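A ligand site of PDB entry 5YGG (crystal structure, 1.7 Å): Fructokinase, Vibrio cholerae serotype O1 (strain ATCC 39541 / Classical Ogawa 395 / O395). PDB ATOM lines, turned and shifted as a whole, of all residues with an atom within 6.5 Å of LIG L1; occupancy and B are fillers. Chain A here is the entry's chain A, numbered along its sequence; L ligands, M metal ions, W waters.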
ATOM      1  N   ASP A  26     -29.387  13.433   2.191  1.00  0.00           N
ATOM      2  CA  ASP A  26     -28.019  13.545   2.672  1.00  0.00           C
ATOM      3  C   ASP A  26     -27.921  13.758   4.164  1.00  0.00           C
ATOM      4  O   ASP A  26     -28.427  14.736   4.701  1.00  0.00           O
ATOM      5  CB  ASP A  26     -27.262  14.665   1.930  1.00  0.00           C
ATOM      6  CG  ASP A  26     -27.915  16.051   2.105  1.00  0.00           C
ATOM      7  OD1 ASP A  26     -29.153  16.177   1.989  1.00  0.00           O
ATOM      8  OD2 ASP A  26     -27.149  17.009   2.326  1.00  0.00           O
ATOM      9  N   VAL A  28     -25.013  14.621   6.757  1.00  0.00           N
ATOM     10  CA  VAL A  28     -23.710  15.252   6.513  1.00  0.00           C
ATOM     11  C   VAL A  28     -23.089  15.706   7.828  1.00  0.00           C
ATOM     12  O   VAL A  28     -23.793  15.972   8.798  1.00  0.00           O
ATOM     13  CB  VAL A  28     -23.803  16.494   5.554  1.00  0.00           C
ATOM     14  CG1 VAL A  28     -24.855  16.284   4.463  1.00  0.00           C
ATOM     15  CG2 VAL A  28     -24.061  17.763   6.297  1.00  0.00           C
ATOM     16  N   VAL A  29     -21.758  15.777   7.850  1.00  0.00           N
ATOM     17  CA  VAL A  29     -21.060  16.398   8.975  1.00  0.00           C
ATOM     18  C   VAL A  29     -20.805  17.847   8.595  1.00  0.00           C
ATOM     19  O   VAL A  29     -20.157  18.131   7.574  1.00  0.00           O
ATOM     20  CB  VAL A  29     -19.736  15.681   9.297  1.00  0.00           C
ATOM     21  CG1 VAL A  29     -18.916  16.492  10.327  1.00  0.00           C
ATOM     22  CG2 VAL A  29     -20.035  14.278   9.795  1.00  0.00           C
ATOM     23  N   ASP A  30     -21.344  18.743   9.410  1.00  0.00           N
ATOM     24  CA  ASP A  30     -21.149  20.189   9.257  1.00  0.00           C
ATOM     25  C   ASP A  30     -19.988  20.647  10.109  1.00  0.00           C
ATOM     26  O   ASP A  30     -20.034  20.493  11.327  1.00  0.00           O
ATOM     27  CB  ASP A  30     -22.398  20.978   9.714  1.00  0.00           C
ATOM     28  CG  ASP A  30     -23.566  20.846   8.759  1.00  0.00           C
ATOM     29  OD1 ASP A  30     -23.348  20.680   7.545  1.00  0.00           O
ATOM     30  OD2 ASP A  30     -24.712  20.954   9.228  1.00  0.00           O
ATOM     31  N   PRO A  43     -23.421  17.088  13.700  1.00  0.00           N
ATOM     32  CA  PRO A  43     -24.260  16.304  12.792  1.00  0.00           C
ATOM     33  C   PRO A  43     -25.251  17.191  12.029  1.00  0.00           C
ATOM     34  O   PRO A  43     -25.753  18.185  12.569  1.00  0.00           O
ATOM     35  CB  PRO A  43     -24.992  15.329  13.731  1.00  0.00           C
ATOM     36  CG  PRO A  43     -25.064  16.083  15.040  1.00  0.00           C
ATOM     37  CD  PRO A  43     -23.858  16.980  15.111  1.00  0.00           C
ATOM     38  N   GLY A  44     -25.492  16.867  10.765  1.00  0.00           N
ATOM     39  CA  GLY A  44     -26.336  17.705   9.927  1.00  0.00           C
ATOM     40  C   GLY A  44     -26.830  17.008   8.678  1.00  0.00           C
ATOM     41  O   GLY A  44     -26.894  15.773   8.627  1.00  0.00           O
ATOM     42  N   GLY A  45     -27.194  17.808   7.676  1.00  0.00           N
ATOM     43  CA  GLY A  45     -27.795  17.308   6.443  1.00  0.00           C
ATOM     44  C   GLY A  45     -29.305  17.455   6.538  1.00  0.00           C
ATOM     45  O   GLY A  45     -29.911  16.898   7.449  1.00  0.00           O
ATOM     46  N   ALA A  46     -29.913  18.192   5.627  1.00  0.00           N
ATOM     47  CA  ALA A  46     -31.296  18.654   5.835  1.00  0.00           C
ATOM     48  C   ALA A  46     -32.282  17.532   6.180  1.00  0.00           C
ATOM     49  O   ALA A  46     -33.005  17.649   7.161  1.00  0.00           O
ATOM     50  CB  ALA A  46     -31.778  19.441   4.624  1.00  0.00           C
ATOM     51  N   PRO A  47     -32.302  16.414   5.408  1.00  0.00           N
ATOM     52  CA  PRO A  47     -33.301  15.413   5.803  1.00  0.00           C
ATOM     53  C   PRO A  47     -32.977  14.746   7.136  1.00  0.00           C
ATOM     54  O   PRO A  47     -33.909  14.344   7.826  1.00  0.00           O
ATOM     55  CB  PRO A  47     -33.286  14.396   4.656  1.00  0.00           C
ATOM     56  CG  PRO A  47     -31.977  14.610   3.943  1.00  0.00           C
ATOM     57  CD  PRO A  47     -31.673  16.085   4.103  1.00  0.00           C
ATOM     58  N   ASN A  49     -31.670  16.381   9.658  1.00  0.00           N
ATOM     59  CA  ASN A  49     -32.142  17.395  10.611  1.00  0.00           C
ATOM     60  C   ASN A  49     -33.649  17.260  10.836  1.00  0.00           C
ATOM     61  O   ASN A  49     -34.118  17.265  11.974  1.00  0.00           O
ATOM     62  CB  ASN A  49     -31.825  18.812  10.117  1.00  0.00           C
ATOM     63  CG  ASN A  49     -30.343  19.055   9.927  1.00  0.00           C
ATOM     64  OD1 ASN A  49     -29.942  19.906   9.113  1.00  0.00           O
ATOM     65  ND2 ASN A  49     -29.530  18.341  10.672  1.00  0.00           N
ATOM     66  N   SER A  99     -20.877  13.049   3.001  1.00  0.00           N
ATOM     67  CA  SER A  99     -20.856  14.480   2.745  1.00  0.00           C
ATOM     68  C   SER A  99     -20.239  15.245   3.907  1.00  0.00           C
ATOM     69  O   SER A  99     -20.592  15.029   5.048  1.00  0.00           O
ATOM     70  CB  SER A  99     -22.278  14.983   2.481  1.00  0.00           C
ATOM     71  OG  SER A  99     -22.272  16.358   2.164  1.00  0.00           O
ATOM     72  N   VAL A 101     -19.349  19.246   5.048  1.00  0.00           N
ATOM     73  CA  VAL A 101     -19.690  20.627   4.716  1.00  0.00           C
ATOM     74  C   VAL A 101     -19.027  21.615   5.658  1.00  0.00           C
ATOM     75  O   VAL A 101     -19.095  21.431   6.870  1.00  0.00           O
ATOM     76  CB  VAL A 101     -21.205  20.819   4.770  1.00  0.00           C
ATOM     77  CG1 VAL A 101     -21.565  22.283   4.614  1.00  0.00           C
ATOM     78  CG2 VAL A 101     -21.870  19.962   3.697  1.00  0.00           C
ATOM     79  N   VAL A 103     -19.045  25.376   7.211  1.00  0.00           N
ATOM     80  CA  VAL A 103     -20.029  26.434   7.391  1.00  0.00           C
ATOM     81  C   VAL A 103     -19.356  27.805   7.570  1.00  0.00           C
ATOM     82  O   VAL A 103     -18.338  27.916   8.248  1.00  0.00           O
ATOM     83  CB  VAL A 103     -20.953  26.130   8.585  1.00  0.00           C
ATOM     84  CG1 VAL A 103     -21.943  27.279   8.826  1.00  0.00           C
ATOM     85  CG2 VAL A 103     -21.713  24.829   8.344  1.00  0.00           C
ATOM     86  N   GLY A 109     -28.169  30.174   5.066  1.00  0.00           N
ATOM     87  CA  GLY A 109     -28.748  29.505   3.925  1.00  0.00           C
ATOM     88  C   GLY A 109     -27.680  28.995   2.979  1.00  0.00           C
ATOM     89  O   GLY A 109     -26.540  28.725   3.397  1.00  0.00           O
ATOM     90  N   PHE A 113     -22.728  27.491   2.980  1.00  0.00           N
ATOM     91  CA  PHE A 113     -22.205  26.127   2.910  1.00  0.00           C
ATOM     92  C   PHE A 113     -21.210  25.884   1.785  1.00  0.00           C
ATOM     93  O   PHE A 113     -21.437  26.293   0.647  1.00  0.00           O
ATOM     94  CB  PHE A 113     -23.362  25.137   2.796  1.00  0.00           C
ATOM     95  CG  PHE A 113     -24.346  25.237   3.926  1.00  0.00           C
ATOM     96  CD1 PHE A 113     -23.986  24.856   5.210  1.00  0.00           C
ATOM     97  CD2 PHE A 113     -25.624  25.732   3.713  1.00  0.00           C
ATOM     98  CE1 PHE A 113     -24.883  24.965   6.260  1.00  0.00           C
ATOM     99  CE2 PHE A 113     -26.531  25.831   4.757  1.00  0.00           C
ATOM    100  CZ  PHE A 113     -26.163  25.452   6.029  1.00  0.00           C
ATOM    101  N   PHE A 115     -19.480  22.574   0.035  1.00  0.00           N
ATOM    102  CA  PHE A 115     -19.537  21.114   0.013  1.00  0.00           C
ATOM    103  C   PHE A 115     -18.194  20.543  -0.439  1.00  0.00           C
ATOM    104  O   PHE A 115     -17.757  20.772  -1.563  1.00  0.00           O
ATOM    105  CB  PHE A 115     -20.676  20.635  -0.909  1.00  0.00           C
ATOM    106  CG  PHE A 115     -22.046  20.959  -0.350  1.00  0.00           C
ATOM    107  CD1 PHE A 115     -22.544  22.254  -0.386  1.00  0.00           C
ATOM    108  CD2 PHE A 115     -22.810  19.977   0.258  1.00  0.00           C
ATOM    109  CE1 PHE A 115     -23.784  22.571   0.150  1.00  0.00           C
ATOM    110  CE2 PHE A 115     -24.047  20.277   0.811  1.00  0.00           C
ATOM    111  CZ  PHE A 115     -24.543  21.582   0.761  1.00  0.00           C
ATOM    112  N   ILE A 144     -31.050  18.332  -2.876  1.00  0.00           N
ATOM    113  CA  ILE A 144     -29.741  17.705  -3.049  1.00  0.00           C
ATOM    114  C   ILE A 144     -29.921  16.235  -3.522  1.00  0.00           C
ATOM    115  O   ILE A 144     -29.104  15.720  -4.303  1.00  0.00           O
ATOM    116  CB  ILE A 144     -28.904  17.780  -1.766  1.00  0.00           C
ATOM    117  CG1 ILE A 144     -28.206  19.144  -1.696  1.00  0.00           C
ATOM    118  CG2 ILE A 144     -27.865  16.648  -1.681  1.00  0.00           C
ATOM    119  CD1 ILE A 144     -27.258  19.270  -0.492  1.00  0.00           C
ATOM    120  N   ASN A 174     -34.573  23.588  -0.651  1.00  0.00           N
ATOM    121  CA  ASN A 174     -33.332  23.682   0.115  1.00  0.00           C
ATOM    122  C   ASN A 174     -32.135  23.753  -0.829  1.00  0.00           C
ATOM    123  O   ASN A 174     -31.227  22.908  -0.784  1.00  0.00           O
ATOM    124  CB  ASN A 174     -33.182  22.469   1.044  1.00  0.00           C
ATOM    125  CG  ASN A 174     -32.941  22.865   2.486  1.00  0.00           C
ATOM    126  OD1 ASN A 174     -32.362  23.916   2.768  1.00  0.00           O
ATOM    127  ND2 ASN A 174     -33.371  22.005   3.405  1.00  0.00           N
ATOM    128  N   ARG A 176     -28.938  24.017  -3.035  1.00  0.00           N
ATOM    129  CA  ARG A 176     -27.487  24.088  -2.887  1.00  0.00           C
ATOM    130  C   ARG A 176     -26.874  23.825  -4.262  1.00  0.00           C
ATOM    131  O   ARG A 176     -26.537  22.691  -4.580  1.00  0.00           O
ATOM    132  CB  ARG A 176     -26.982  23.078  -1.858  1.00  0.00           C
ATOM    133  CG  ARG A 176     -27.712  23.122  -0.518  1.00  0.00           C
ATOM    134  CD  ARG A 176     -27.341  24.331   0.368  1.00  0.00           C
ATOM    135  NE  ARG A 176     -27.887  24.109   1.699  1.00  0.00           N
ATOM    136  CZ  ARG A 176     -29.078  24.531   2.107  1.00  0.00           C
ATOM    137  NH1 ARG A 176     -29.849  25.242   1.304  1.00  0.00           N
ATOM    138  NH2 ARG A 176     -29.494  24.251   3.338  1.00  0.00           N
ATOM    139  N   THR A 262     -27.922  27.997  11.131  1.00  0.00           N
ATOM    140  CA  THR A 262     -27.818  26.673  10.540  1.00  0.00           C
ATOM    141  C   THR A 262     -28.952  25.770  11.019  1.00  0.00           C
ATOM    142  O   THR A 262     -29.121  25.592  12.229  1.00  0.00           O
ATOM    143  CB  THR A 262     -26.473  25.986  10.868  1.00  0.00           C
ATOM    144  OG1 THR A 262     -25.389  26.821  10.479  1.00  0.00           O
ATOM    145  CG2 THR A 262     -26.376  24.649  10.141  1.00  0.00           C
ATOM    146  N   GLY A 263     -29.717  25.217  10.081  1.00  0.00           N
ATOM    147  CA  GLY A 263     -30.779  24.295  10.428  1.00  0.00           C
ATOM    148  C   GLY A 263     -32.146  24.872  10.760  1.00  0.00           C
ATOM    149  O   GLY A 263     -33.076  24.097  11.007  1.00  0.00           O
ATOM    150  N   ALA A 264     -32.286  26.200  10.797  1.00  0.00           N
ATOM    151  CA  ALA A 264     -33.577  26.823  11.144  1.00  0.00           C
ATOM    152  C   ALA A 264     -34.733  26.330  10.252  1.00  0.00           C
ATOM    153  O   ALA A 264     -35.815  25.995  10.736  1.00  0.00           O
ATOM    154  CB  ALA A 264     -33.481  28.367  11.072  1.00  0.00           C
ATOM    155  N   GLY A 265     -34.501  26.294   8.949  1.00  0.00           N
ATOM    156  CA  GLY A 265     -35.530  25.884   8.005  1.00  0.00           C
ATOM    157  C   GLY A 265     -35.931  24.425   8.168  1.00  0.00           C
ATOM    158  O   GLY A 265     -37.094  24.071   7.972  1.00  0.00           O
ATOM    159  N   ASP A 266     -34.965  23.574   8.493  1.00  0.00           N
ATOM    160  CA  ASP A 266     -35.257  22.146   8.672  1.00  0.00           C
ATOM    161  C   ASP A 266     -36.022  21.923   9.966  1.00  0.00           C
ATOM    162  O   ASP A 266     -36.871  21.039  10.062  1.00  0.00           O
ATOM    163  CB  ASP A 266     -33.966  21.327   8.681  1.00  0.00           C
ATOM    164  CG  ASP A 266     -33.176  21.470   7.397  1.00  0.00           C
ATOM    165  OD1 ASP A 266     -33.793  21.692   6.321  1.00  0.00           O
ATOM    166  OD2 ASP A 266     -31.931  21.351   7.444  1.00  0.00           O
ATOM    167  N   ALA A 308     -27.005  22.314  13.400  1.00  0.00           N
ATOM    168  CA  ALA A 308     -28.381  22.202  12.932  1.00  0.00           C
ATOM    169  C   ALA A 308     -29.282  21.456  13.927  1.00  0.00           C
ATOM    170  O   ALA A 308     -30.459  21.782  14.057  1.00  0.00           O
ATOM    171  CB  ALA A 308     -28.422  21.495  11.585  1.00  0.00           C
HETATM  172  C1  LIG L   1     -27.077  20.205   3.210  1.00  0.00           C
HETATM  173  C2  LIG L   1     -27.012  21.327   4.280  1.00  0.00           C
HETATM  174  C3  LIG L   1     -26.357  20.866   5.583  1.00  0.00           C
HETATM  175  C4  LIG L   1     -26.982  21.530   6.561  1.00  0.00           C
HETATM  176  C5  LIG L   1     -28.512  21.636   6.009  1.00  0.00           C
HETATM  177  C6  LIG L   1     -29.248  22.844   6.543  1.00  0.00           C
HETATM  178  O1  LIG L   1     -28.061  19.219   3.508  1.00  0.00           O
HETATM  179  O2  LIG L   1     -26.414  22.360   3.792  1.00  0.00           O
HETATM  180  O3  LIG L   1     -24.921  21.242   5.506  1.00  0.00           O
HETATM  181  O4  LIG L   1     -27.000  20.836   7.839  1.00  0.00           O
HETATM  182  O5  LIG L   1     -28.461  21.728   4.708  1.00  0.00           O
HETATM  183  O6  LIG L   1     -30.493  22.912   5.851  1.00  0.00           O
HETATM  184  P1  LG2 L   2     -34.910  29.217   5.485  1.00  0.00           P
HETATM  185  O1  LG2 L   2     -34.507  30.288   4.459  1.00  0.00           O
HETATM  186  O2  LG2 L   2     -33.961  28.093   5.403  1.00  0.00           O
HETATM  187  O3  LG2 L   2     -36.332  28.699   5.183  1.00  0.00           O
HETATM  188  P2  LG2 L   2     -35.754  31.198   7.422  1.00  0.00           P
HETATM  189  O4  LG2 L   2     -34.780  32.401   7.568  1.00  0.00           O
HETATM  190  O5  LG2 L   2     -36.795  31.556   6.386  1.00  0.00           O
HETATM  191  O6  LG2 L   2     -34.913  29.838   6.972  1.00  0.00           O
HETATM  192  O7  LG2 L   2     -36.457  30.919   8.796  1.00  0.00           O
HETATM  193  C1  LG2 L   2     -36.864  29.602   9.097  1.00  0.00           C
HETATM  194  C2  LG2 L   2     -37.858  29.622  10.043  1.00  0.00           C
HETATM  195  O8  LG2 L   2     -37.235  29.672  11.429  1.00  0.00           O
HETATM  196  C3  LG2 L   2     -38.743  30.916   9.937  1.00  0.00           C
HETATM  197  O9  LG2 L   2     -39.995  30.648   9.201  1.00  0.00           O
HETATM  198  C4  LG2 L   2     -39.009  31.222  11.141  1.00  0.00           C
HETATM  199  O10 LG2 L   2     -40.217  30.509  11.582  1.00  0.00           O
HETATM  200  C5  LG2 L   2     -37.708  30.752  12.017  1.00  0.00           C
HETATM  201  N1  LG2 L   2     -36.741  31.777  12.064  1.00  0.00           N
HETATM  202  C6  LG2 L   2     -35.641  32.096  11.344  1.00  0.00           C
HETATM  203  N2  LG2 L   2     -35.116  33.229  11.871  1.00  0.00           N
HETATM  204  C7  LG2 L   2     -35.905  33.615  12.922  1.00  0.00           C
HETATM  205  C8  LG2 L   2     -35.821  34.684  13.794  1.00  0.00           C
HETATM  206  N3  LG2 L   2     -35.019  35.735  13.993  1.00  0.00           N
HETATM  207  N4  LG2 L   2     -36.755  34.833  14.776  1.00  0.00           N
HETATM  208  C9  LG2 L   2     -37.777  33.921  14.885  1.00  0.00           C
HETATM  209  N5  LG2 L   2     -37.863  32.872  14.038  1.00  0.00           N
HETATM  210  C10 LG2 L   2     -36.917  32.715  13.046  1.00  0.00           C
HETATM  211 CA    CA M   1     -33.437  25.805   3.964  1.00  0.00          CA
HETATM  212  O   HOH W   1     -29.490  26.216   7.206  1.00  0.00           O
HETATM  213  O   HOH W   2     -30.238  18.780   1.760  1.00  0.00           O
HETATM  214  O   HOH W   3     -32.076  24.589   7.506  1.00  0.00           O
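The side-chain carboxylate of Asp 30 sits at hydrogen-bond distance from an oxygen (O3) of LIG L1 (2.6 Å).
The side-chain carboxylate of Asp 266 is in hydrogen-bond range of an oxygen (O6) of LIG L1 (2.7 Å).
An oxygen (O1) of LIG L1 is in hydrogen-bond range of the side-chain carboxylate (OD2) of Asp 26 (2.7 Å).
An oxygen (O1) of LIG L1 lies within hydrogen-bond range of the backbone NH (N) of Ala 46, 3.0 Å away.
An oxygen (O6) of LIG L1 sits at hydrogen-bond distance from the guanidinium group (NH2) of Arg 176, 3.0 Å away.
The backbone NH (N) of Gly 45 sits at hydrogen-bond distance from an oxygen (O4) of LIG L1, 3.0 Å away.
OD1 of Asn 49 lies within hydrogen-bond range of O4 of LIG L1.
The side-chain carboxylate of Asp 266 sits close to the side-chain amide oxygen of Asn 49, 3.0 Å away.
ND2 of Asn 174 lies within hydrogen-bond range of OD1 of Asp 266, 3.0 Å away.
The guanidinium group (NH1) of Arg 176 lies within hydrogen-bond range of the backbone carbonyl oxygen (O) of Asn 174, 3.4 Å away.
The backbone carbonyl oxygen of Gly 45 lies close to the side-chain amide oxygen of Asn 49 (3.4 Å).
The backbone NH (N) of Val 101 lies within hydrogen-bond range of the backbone carbonyl oxygen (O) of Val 29 (2.9 Å).
N of Gly 44 lies within hydrogen-bond range of O of Val 28 (2.7 Å).
CG2 of Val 28 touches O3 of LIG L1, 3.7 Å away.
Gly 44 touches LIG L1.
Val 101 touches LIG L1.
Phe 113 touches LIG L1.
Phe 115 touches LIG L1.
Ile 144 touches LIG L1 (CD1 to C1, 3.8 Å).
Asn 174 touches LIG L1 (OD1 to O6, 3.7 Å).
Hydrophobic or aromatic side chains within 4 Å of LIG L1: Val 28, Ala 46, Val 101, Phe 113, Phe 115 and Ile 144.
The nearest printed residue that does not touch LIG L1 is Ala 308 (4.1 Å).
Water W2 lies within hydrogen-bond range of an oxygen (O1) of LIG L1 (2.8 Å) and the side-chain carboxylate (OD1) of Asp 26 (2.8 Å).
Water W3 lies within hydrogen-bond range of O6 of LIG L1 (2.8 Å), N of Asp 266 (3.2 Å) and N of Gly 265 (3.3 Å).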
